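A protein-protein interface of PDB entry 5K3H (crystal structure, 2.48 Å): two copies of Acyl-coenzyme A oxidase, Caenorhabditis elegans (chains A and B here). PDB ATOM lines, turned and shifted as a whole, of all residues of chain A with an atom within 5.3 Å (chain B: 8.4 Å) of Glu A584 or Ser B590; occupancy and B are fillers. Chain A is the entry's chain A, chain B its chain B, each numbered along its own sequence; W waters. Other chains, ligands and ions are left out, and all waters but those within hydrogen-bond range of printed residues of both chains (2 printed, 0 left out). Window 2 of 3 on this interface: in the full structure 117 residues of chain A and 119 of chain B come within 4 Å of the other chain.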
ATOM      1  N   ARG A 501      -9.760  26.600  14.832  1.00  0.00           N
ATOM      2  CA  ARG A 501     -10.811  26.722  15.844  1.00  0.00           C
ATOM      3  C   ARG A 501     -10.227  27.087  17.193  1.00  0.00           C
ATOM      4  O   ARG A 501     -10.687  28.028  17.851  1.00  0.00           O
ATOM      5  CB  ARG A 501     -11.598  25.418  15.942  1.00  0.00           C
ATOM      6  CG  ARG A 501     -12.987  25.568  16.527  1.00  0.00           C
ATOM      7  CD  ARG A 501     -13.598  24.204  16.731  1.00  0.00           C
ATOM      8  NE  ARG A 501     -13.186  23.615  18.001  1.00  0.00           N
ATOM      9  CZ  ARG A 501     -13.835  23.769  19.147  1.00  0.00           C
ATOM     10  NH1 ARG A 501     -14.944  24.504  19.196  1.00  0.00           N
ATOM     11  NH2 ARG A 501     -13.372  23.187  20.250  1.00  0.00           N
ATOM     12  N   LYS A 505     -10.659  30.647  19.185  1.00  0.00           N
ATOM     13  CA  LYS A 505     -11.330  30.543  20.474  1.00  0.00           C
ATOM     14  C   LYS A 505     -10.479  31.153  21.585  1.00  0.00           C
ATOM     15  O   LYS A 505     -10.965  31.962  22.391  1.00  0.00           O
ATOM     16  CB  LYS A 505     -11.663  29.082  20.762  1.00  0.00           C
ATOM     17  CG  LYS A 505     -12.357  28.850  22.077  1.00  0.00           C
ATOM     18  CD  LYS A 505     -12.504  27.361  22.356  1.00  0.00           C
ATOM     19  CE  LYS A 505     -13.189  27.091  23.695  1.00  0.00           C
ATOM     20  NZ  LYS A 505     -13.702  25.696  23.788  1.00  0.00           N
ATOM     21  N   ALA A 579      -7.865  14.315  19.426  1.00  0.00           N
ATOM     22  CA  ALA A 579      -9.246  14.033  19.035  1.00  0.00           C
ATOM     23  C   ALA A 579     -10.258  14.922  19.757  1.00  0.00           C
ATOM     24  O   ALA A 579     -11.324  15.216  19.199  1.00  0.00           O
ATOM     25  CB  ALA A 579      -9.561  12.560  19.273  1.00  0.00           C
ATOM     26  N   THR A 580      -9.978  15.303  21.008  1.00  0.00           N
ATOM     27  CA  THR A 580     -10.872  16.191  21.761  1.00  0.00           C
ATOM     28  C   THR A 580     -11.274  17.426  20.961  1.00  0.00           C
ATOM     29  O   THR A 580     -12.441  17.838  20.964  1.00  0.00           O
ATOM     30  CB  THR A 580     -10.188  16.643  23.048  1.00  0.00           C
ATOM     31  OG1 THR A 580     -10.098  15.547  23.964  1.00  0.00           O
ATOM     32  CG2 THR A 580     -10.955  17.798  23.669  1.00  0.00           C
ATOM     33  N   TYR A 581     -10.296  18.078  20.337  1.00  0.00           N
ATOM     34  CA  TYR A 581     -10.611  19.259  19.557  1.00  0.00           C
ATOM     35  C   TYR A 581     -11.446  18.911  18.343  1.00  0.00           C
ATOM     36  O   TYR A 581     -12.314  19.693  17.951  1.00  0.00           O
ATOM     37  CB  TYR A 581      -9.330  19.975  19.159  1.00  0.00           C
ATOM     38  CG  TYR A 581      -8.495  20.346  20.366  1.00  0.00           C
ATOM     39  CD1 TYR A 581      -8.850  21.422  21.176  1.00  0.00           C
ATOM     40  CD2 TYR A 581      -7.347  19.634  20.686  1.00  0.00           C
ATOM     41  CE1 TYR A 581      -8.087  21.775  22.274  1.00  0.00           C
ATOM     42  CE2 TYR A 581      -6.573  19.980  21.785  1.00  0.00           C
ATOM     43  CZ  TYR A 581      -6.950  21.046  22.577  1.00  0.00           C
ATOM     44  OH  TYR A 581      -6.182  21.389  23.668  1.00  0.00           O
ATOM     45  N   ALA A 582     -11.251  17.716  17.780  1.00  0.00           N
ATOM     46  CA  ALA A 582     -11.987  17.320  16.581  1.00  0.00           C
ATOM     47  C   ALA A 582     -13.439  16.977  16.897  1.00  0.00           C
ATOM     48  O   ALA A 582     -14.334  17.259  16.099  1.00  0.00           O
ATOM     49  CB  ALA A 582     -11.280  16.139  15.914  1.00  0.00           C
ATOM     50  N   LEU A 583     -13.693  16.388  18.061  1.00  0.00           N
ATOM     51  CA  LEU A 583     -15.034  15.977  18.463  1.00  0.00           C
ATOM     52  C   LEU A 583     -15.882  17.123  19.017  1.00  0.00           C
ATOM     53  O   LEU A 583     -17.109  17.000  19.059  1.00  0.00           O
ATOM     54  CB  LEU A 583     -14.935  14.891  19.537  1.00  0.00           C
ATOM     55  CG  LEU A 583     -14.241  13.573  19.210  1.00  0.00           C
ATOM     56  CD1 LEU A 583     -13.866  12.877  20.502  1.00  0.00           C
ATOM     57  CD2 LEU A 583     -15.147  12.686  18.391  1.00  0.00           C
ATOM     58  N   GLU A 584     -15.259  18.206  19.490  1.00  0.00           N
ATOM     59  CA  GLU A 584     -15.962  19.178  20.330  1.00  0.00           C
ATOM     60  C   GLU A 584     -17.095  19.898  19.597  1.00  0.00           C
ATOM     61  O   GLU A 584     -18.147  20.163  20.191  1.00  0.00           O
ATOM     62  CB  GLU A 584     -14.979  20.201  20.886  1.00  0.00           C
ATOM     63  CG  GLU A 584     -15.101  20.349  22.381  1.00  0.00           C
ATOM     64  CD  GLU A 584     -14.233  21.457  22.900  1.00  0.00           C
ATOM     65  OE1 GLU A 584     -13.078  21.591  22.398  1.00  0.00           O
ATOM     66  OE2 GLU A 584     -14.702  22.164  23.835  1.00  0.00           O
ATOM     67  N   ASP A 585     -16.874  20.324  18.357  1.00  0.00           N
ATOM     68  CA  ASP A 585     -17.946  20.958  17.603  1.00  0.00           C
ATOM     69  C   ASP A 585     -18.666  19.964  16.698  1.00  0.00           C
ATOM     70  O   ASP A 585     -19.346  20.373  15.754  1.00  0.00           O
ATOM     71  CB  ASP A 585     -17.417  22.137  16.778  1.00  0.00           C
ATOM     72  CG  ASP A 585     -16.294  21.730  15.833  1.00  0.00           C
ATOM     73  OD1 ASP A 585     -15.783  20.602  16.011  1.00  0.00           O
ATOM     74  OD2 ASP A 585     -15.895  22.532  14.953  1.00  0.00           O
ATOM     75  N   GLY A 586     -18.522  18.667  16.954  1.00  0.00           N
ATOM     76  CA  GLY A 586     -19.090  17.708  16.033  1.00  0.00           C
ATOM     77  C   GLY A 586     -18.467  17.704  14.653  1.00  0.00           C
ATOM     78  O   GLY A 586     -19.074  17.175  13.718  1.00  0.00           O
ATOM     79  N   LEU B 576     -10.562  16.932  32.080  1.00  0.00           N
ATOM     80  CA  LEU B 576     -10.089  17.532  30.837  1.00  0.00           C
ATOM     81  C   LEU B 576      -9.071  16.632  30.159  1.00  0.00           C
ATOM     82  O   LEU B 576      -9.040  16.548  28.926  1.00  0.00           O
ATOM     83  CB  LEU B 576      -9.506  18.919  31.104  1.00  0.00           C
ATOM     84  CG  LEU B 576      -9.477  19.969  29.976  1.00  0.00           C
ATOM     85  CD1 LEU B 576     -10.854  20.274  29.388  1.00  0.00           C
ATOM     86  CD2 LEU B 576      -8.850  21.248  30.500  1.00  0.00           C
ATOM     87  N   ALA B 579     -10.868  13.866  28.082  1.00  0.00           N
ATOM     88  CA  ALA B 579     -12.075  14.477  27.532  1.00  0.00           C
ATOM     89  C   ALA B 579     -12.616  13.723  26.322  1.00  0.00           C
ATOM     90  O   ALA B 579     -13.839  13.655  26.126  1.00  0.00           O
ATOM     91  CB  ALA B 579     -11.791  15.936  27.171  1.00  0.00           C
ATOM     92  N   THR B 580     -11.728  13.181  25.481  1.00  0.00           N
ATOM     93  CA  THR B 580     -12.162  12.423  24.305  1.00  0.00           C
ATOM     94  C   THR B 580     -13.175  11.336  24.658  1.00  0.00           C
ATOM     95  O   THR B 580     -14.216  11.207  24.008  1.00  0.00           O
ATOM     96  CB  THR B 580     -10.944  11.823  23.601  1.00  0.00           C
ATOM     97  OG1 THR B 580     -10.198  12.881  22.985  1.00  0.00           O
ATOM     98  CG2 THR B 580     -11.354  10.805  22.534  1.00  0.00           C
ATOM     99  N   ALA B 582     -15.231  11.246  27.067  1.00  0.00           N
ATOM    100  CA  ALA B 582     -16.503  11.831  27.499  1.00  0.00           C
ATOM    101  C   ALA B 582     -17.294  12.383  26.321  1.00  0.00           C
ATOM    102  O   ALA B 582     -18.530  12.318  26.310  1.00  0.00           O
ATOM    103  CB  ALA B 582     -16.256  12.929  28.541  1.00  0.00           C
ATOM    104  N   LEU B 583     -16.590  12.932  25.326  1.00  0.00           N
ATOM    105  CA  LEU B 583     -17.230  13.543  24.176  1.00  0.00           C
ATOM    106  C   LEU B 583     -17.680  12.513  23.148  1.00  0.00           C
ATOM    107  O   LEU B 583     -18.629  12.778  22.399  1.00  0.00           O
ATOM    108  CB  LEU B 583     -16.256  14.526  23.511  1.00  0.00           C
ATOM    109  CG  LEU B 583     -15.781  15.778  24.278  1.00  0.00           C
ATOM    110  CD1 LEU B 583     -14.515  16.324  23.654  1.00  0.00           C
ATOM    111  CD2 LEU B 583     -16.854  16.867  24.286  1.00  0.00           C
ATOM    112  N   GLU B 584     -17.043  11.338  23.097  1.00  0.00           N
ATOM    113  CA  GLU B 584     -17.201  10.493  21.917  1.00  0.00           C
ATOM    114  C   GLU B 584     -18.643  10.053  21.721  1.00  0.00           C
ATOM    115  O   GLU B 584     -19.155  10.062  20.593  1.00  0.00           O
ATOM    116  CB  GLU B 584     -16.302   9.268  21.984  1.00  0.00           C
ATOM    117  CG  GLU B 584     -15.535   9.082  20.693  1.00  0.00           C
ATOM    118  CD  GLU B 584     -14.782   7.761  20.650  1.00  0.00           C
ATOM    119  OE1 GLU B 584     -14.138   7.409  21.689  1.00  0.00           O
ATOM    120  OE2 GLU B 584     -14.893   7.065  19.592  1.00  0.00           O
ATOM    121  N   GLY B 586     -21.241  11.614  22.985  1.00  0.00           N
ATOM    122  CA  GLY B 586     -22.083  12.723  23.392  1.00  0.00           C
ATOM    123  C   GLY B 586     -22.451  12.777  24.862  1.00  0.00           C
ATOM    124  O   GLY B 586     -23.366  13.512  25.239  1.00  0.00           O
ATOM    125  N   PHE B 587     -21.749  12.043  25.722  1.00  0.00           N
ATOM    126  CA  PHE B 587     -22.073  12.096  27.145  1.00  0.00           C
ATOM    127  C   PHE B 587     -21.807  13.485  27.717  1.00  0.00           C
ATOM    128  O   PHE B 587     -22.483  13.908  28.661  1.00  0.00           O
ATOM    129  CB  PHE B 587     -21.305  11.019  27.915  1.00  0.00           C
ATOM    130  CG  PHE B 587     -21.844  10.772  29.296  1.00  0.00           C
ATOM    131  CD1 PHE B 587     -23.031  10.053  29.466  1.00  0.00           C
ATOM    132  CD2 PHE B 587     -21.188  11.257  30.431  1.00  0.00           C
ATOM    133  CE1 PHE B 587     -23.552   9.812  30.736  1.00  0.00           C
ATOM    134  CE2 PHE B 587     -21.715  11.021  31.715  1.00  0.00           C
ATOM    135  CZ  PHE B 587     -22.892  10.302  31.863  1.00  0.00           C
ATOM    136  N   MET B 588     -20.771  14.171  27.227  1.00  0.00           N
ATOM    137  CA  MET B 588     -20.525  15.586  27.528  1.00  0.00           C
ATOM    138  C   MET B 588     -20.641  16.443  26.269  1.00  0.00           C
ATOM    139  O   MET B 588     -20.277  16.025  25.163  1.00  0.00           O
ATOM    140  CB  MET B 588     -19.132  15.815  28.146  1.00  0.00           C
ATOM    141  CG  MET B 588     -19.067  15.666  29.653  1.00  0.00           C
ATOM    142  SD  MET B 588     -17.454  16.015  30.447  1.00  0.00           S
ATOM    143  CE  MET B 588     -17.207  17.769  30.232  1.00  0.00           C
ATOM    144  N   SER B 589     -21.108  17.666  26.458  1.00  0.00           N
ATOM    145  CA  SER B 589     -21.153  18.656  25.393  1.00  0.00           C
ATOM    146  C   SER B 589     -19.917  19.548  25.444  1.00  0.00           C
ATOM    147  O   SER B 589     -19.174  19.592  26.434  1.00  0.00           O
ATOM    148  CB  SER B 589     -22.395  19.522  25.527  1.00  0.00           C
ATOM    149  OG  SER B 589     -22.364  20.156  26.803  1.00  0.00           O
ATOM    150  N   SER B 590     -19.713  20.280  24.350  1.00  0.00           N
ATOM    151  CA  SER B 590     -18.674  21.299  24.310  1.00  0.00           C
ATOM    152  C   SER B 590     -18.871  22.328  25.421  1.00  0.00           C
ATOM    153  O   SER B 590     -17.899  22.812  26.013  1.00  0.00           O
ATOM    154  CB  SER B 590     -18.666  21.966  22.935  1.00  0.00           C
ATOM    155  OG  SER B 590     -17.669  22.976  22.866  1.00  0.00           O
ATOM    156  N   THR B 591     -20.124  22.705  25.689  1.00  0.00           N
ATOM    157  CA  THR B 591     -20.405  23.660  26.758  1.00  0.00           C
ATOM    158  C   THR B 591     -19.972  23.136  28.123  1.00  0.00           C
ATOM    159  O   THR B 591     -19.383  23.873  28.917  1.00  0.00           O
ATOM    160  CB  THR B 591     -21.890  24.001  26.766  1.00  0.00           C
ATOM    161  OG1 THR B 591     -22.177  24.822  25.634  1.00  0.00           O
ATOM    162  CG2 THR B 591     -22.249  24.763  28.021  1.00  0.00           C
ATOM    163  N   GLN B 592     -20.266  21.875  28.421  1.00  0.00           N
ATOM    164  CA  GLN B 592     -19.812  21.300  29.681  1.00  0.00           C
ATOM    165  C   GLN B 592     -18.298  21.213  29.747  1.00  0.00           C
ATOM    166  O   GLN B 592     -17.718  21.370  30.821  1.00  0.00           O
ATOM    167  CB  GLN B 592     -20.412  19.909  29.868  1.00  0.00           C
ATOM    168  CG  GLN B 592     -21.861  19.911  30.275  1.00  0.00           C
ATOM    169  CD  GLN B 592     -22.434  18.525  30.287  1.00  0.00           C
ATOM    170  OE1 GLN B 592     -22.323  17.793  29.296  1.00  0.00           O
ATOM    171  NE2 GLN B 592     -23.077  18.151  31.392  1.00  0.00           N
ATOM    172  N   LEU B 593     -17.640  20.964  28.619  1.00  0.00           N
ATOM    173  CA  LEU B 593     -16.186  20.935  28.625  1.00  0.00           C
ATOM    174  C   LEU B 593     -15.619  22.325  28.835  1.00  0.00           C
ATOM    175  O   LEU B 593     -14.567  22.473  29.456  1.00  0.00           O
ATOM    176  CB  LEU B 593     -15.654  20.308  27.333  1.00  0.00           C
ATOM    177  CG  LEU B 593     -14.241  19.718  27.392  1.00  0.00           C
ATOM    178  CD1 LEU B 593     -14.119  18.585  28.435  1.00  0.00           C
ATOM    179  CD2 LEU B 593     -13.762  19.260  25.990  1.00  0.00           C
ATOM    180  N   ASP B 594     -16.291  23.356  28.316  1.00  0.00           N
ATOM    181  CA  ASP B 594     -15.883  24.727  28.604  1.00  0.00           C
ATOM    182  C   ASP B 594     -16.070  25.069  30.077  1.00  0.00           C
ATOM    183  O   ASP B 594     -15.283  25.828  30.647  1.00  0.00           O
ATOM    184  CB  ASP B 594     -16.672  25.694  27.725  1.00  0.00           C
ATOM    185  CG  ASP B 594     -16.219  25.665  26.268  1.00  0.00           C
ATOM    186  OD1 ASP B 594     -15.067  25.215  25.999  1.00  0.00           O
ATOM    187  OD2 ASP B 594     -17.015  26.107  25.397  1.00  0.00           O
ATOM    188  N   TYR B 595     -17.123  24.546  30.708  1.00  0.00           N
ATOM    189  CA  TYR B 595     -17.267  24.706  32.151  1.00  0.00           C
ATOM    190  C   TYR B 595     -16.083  24.092  32.873  1.00  0.00           C
ATOM    191  O   TYR B 595     -15.520  24.697  33.788  1.00  0.00           O
ATOM    192  CB  TYR B 595     -18.580  24.074  32.623  1.00  0.00           C
ATOM    193  CG  TYR B 595     -18.787  24.013  34.141  1.00  0.00           C
ATOM    194  CD1 TYR B 595     -19.427  25.038  34.830  1.00  0.00           C
ATOM    195  CD2 TYR B 595     -18.367  22.906  34.876  1.00  0.00           C
ATOM    196  CE1 TYR B 595     -19.621  24.974  36.206  1.00  0.00           C
ATOM    197  CE2 TYR B 595     -18.559  22.835  36.252  1.00  0.00           C
ATOM    198  CZ  TYR B 595     -19.183  23.868  36.914  1.00  0.00           C
ATOM    199  OH  TYR B 595     -19.364  23.771  38.288  1.00  0.00           O
ATOM    200  N   VAL B 596     -15.662  22.904  32.433  1.00  0.00           N
ATOM    201  CA  VAL B 596     -14.577  22.191  33.095  1.00  0.00           C
ATOM    202  C   VAL B 596     -13.284  22.994  32.999  1.00  0.00           C
ATOM    203  O   VAL B 596     -12.530  23.085  33.972  1.00  0.00           O
ATOM    204  CB  VAL B 596     -14.427  20.778  32.490  1.00  0.00           C
ATOM    205  CG1 VAL B 596     -13.194  20.085  33.043  1.00  0.00           C
ATOM    206  CG2 VAL B 596     -15.667  19.943  32.781  1.00  0.00           C
ATOM    207  N   ARG B 597     -13.030  23.610  31.836  1.00  0.00           N
ATOM    208  CA  ARG B 597     -11.852  24.460  31.652  1.00  0.00           C
ATOM    209  C   ARG B 597     -11.882  25.680  32.563  1.00  0.00           C
ATOM    210  O   ARG B 597     -10.862  26.050  33.151  1.00  0.00           O
ATOM    211  CB  ARG B 597     -11.744  24.912  30.198  1.00  0.00           C
ATOM    212  CG  ARG B 597     -11.499  23.812  29.225  1.00  0.00           C
ATOM    213  CD  ARG B 597     -11.492  24.336  27.802  1.00  0.00           C
ATOM    214  NE  ARG B 597     -11.169  23.279  26.850  1.00  0.00           N
ATOM    215  CZ  ARG B 597     -11.990  22.827  25.902  1.00  0.00           C
ATOM    216  NH1 ARG B 597     -13.206  23.354  25.759  1.00  0.00           N
ATOM    217  NH2 ARG B 597     -11.578  21.858  25.079  1.00  0.00           N
HETATM  218  O   HOH W   1      -8.644  21.214  25.696  1.00  0.00           O
HETATM  219  O   HOH W   2     -11.004  24.822  23.856  1.00  0.00           O
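OE2 of Glu A584 lies within salt-bridge range of NH1 of Arg B597. NH1 of Arg B597 sits close to NZ of Lys A505 (3.1 Å). The side-chain amino group (NZ) of Lys A505 is in salt-bridge range of the side-chain carboxylate (OD1) of Asp B594 (2.6 Å). The side-chain hydroxyl (OG1) of Thr B580 is in hydrogen-bond range of the side-chain hydroxyl (OG1) of Thr A580, at 2.8 Å. The side-chain carboxylate (OE2) of Glu A584 sits at hydrogen-bond distance from the side-chain hydroxyl (OG) of Ser B590, at 3.2 Å.
OE1 of Glu A584 is in salt-bridge range of NH2 of Arg A501 (2.7 Å). The side-chain carboxylate (OD1) of Asp B594 is in salt-bridge range of the guanidinium group (NH1) of Arg B597 (2.6 Å). OE2 of Glu A584 lies within salt-bridge range of NZ of Lys A505 (3.7 Å).
Ala A579 touches Thr B580. Thr A580 touches Ala B579. Thr A580 touches Leu B583. CG2 of Thr A580 touches CD2 of Leu B593, 3.9 Å away. Thr B580 touches Leu A583 (CG2 to CD1, 3.8 Å). OE2 of Glu A584 touches CD2 of Leu B593, at 3.7 Å. Glu A584 touches Asp B594 (OE2 to OD1, 3.8 Å).
Glu A584 touches just these residues of chain B: Ser B590 (3.2 Å), Leu B593 (3.7 Å), Asp B594 (3.8 Å) and Arg B597 (2.7 Å). Of the printed residues of chain A, Ser B590 touches Glu A584 (3.2 Å). Printed residues of chain A within 4 Å of Leu B593: Thr A580 and Glu A584. Printed residues of chain A within 4 Å of Asp B594: Lys A505 and Glu A584. Arg A501 touches none of the printed residues of chain B. Leu B576 touches none of the printed residues of chain A. The nearest residue of chain A that does not touch Ser B590 is Arg A501 (4.8 Å).
Of the 10 printed residues of chain A, 5 touch a printed residue of chain B. Among the printed residues, 12 pairs touch across the chains. Among the printed residues, Asp or Glu carboxylates within 4 Å of a Lys or Arg side-chain nitrogen of the other chain: Lys A505 with Asp B594 and Glu A584 with Arg B597.
Ala A579 touches Thr B580, and with the chains exchanged Thr A580 touches Ala B579. Thr B580 touches its own counterpart, Thr A580. Thr A580 touches Leu B583, and with the chains exchanged Leu A583 touches Thr B580.
Water W2 lies within hydrogen-bond range of the side-chain amino group (NZ) of Lys A505 (2.8 Å) and the guanidinium group (NH2) of Arg B597 (3.3 Å). Water W1 bridges the guanidinium group of Arg B597 and the side-chain hydroxyl of Tyr A581.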
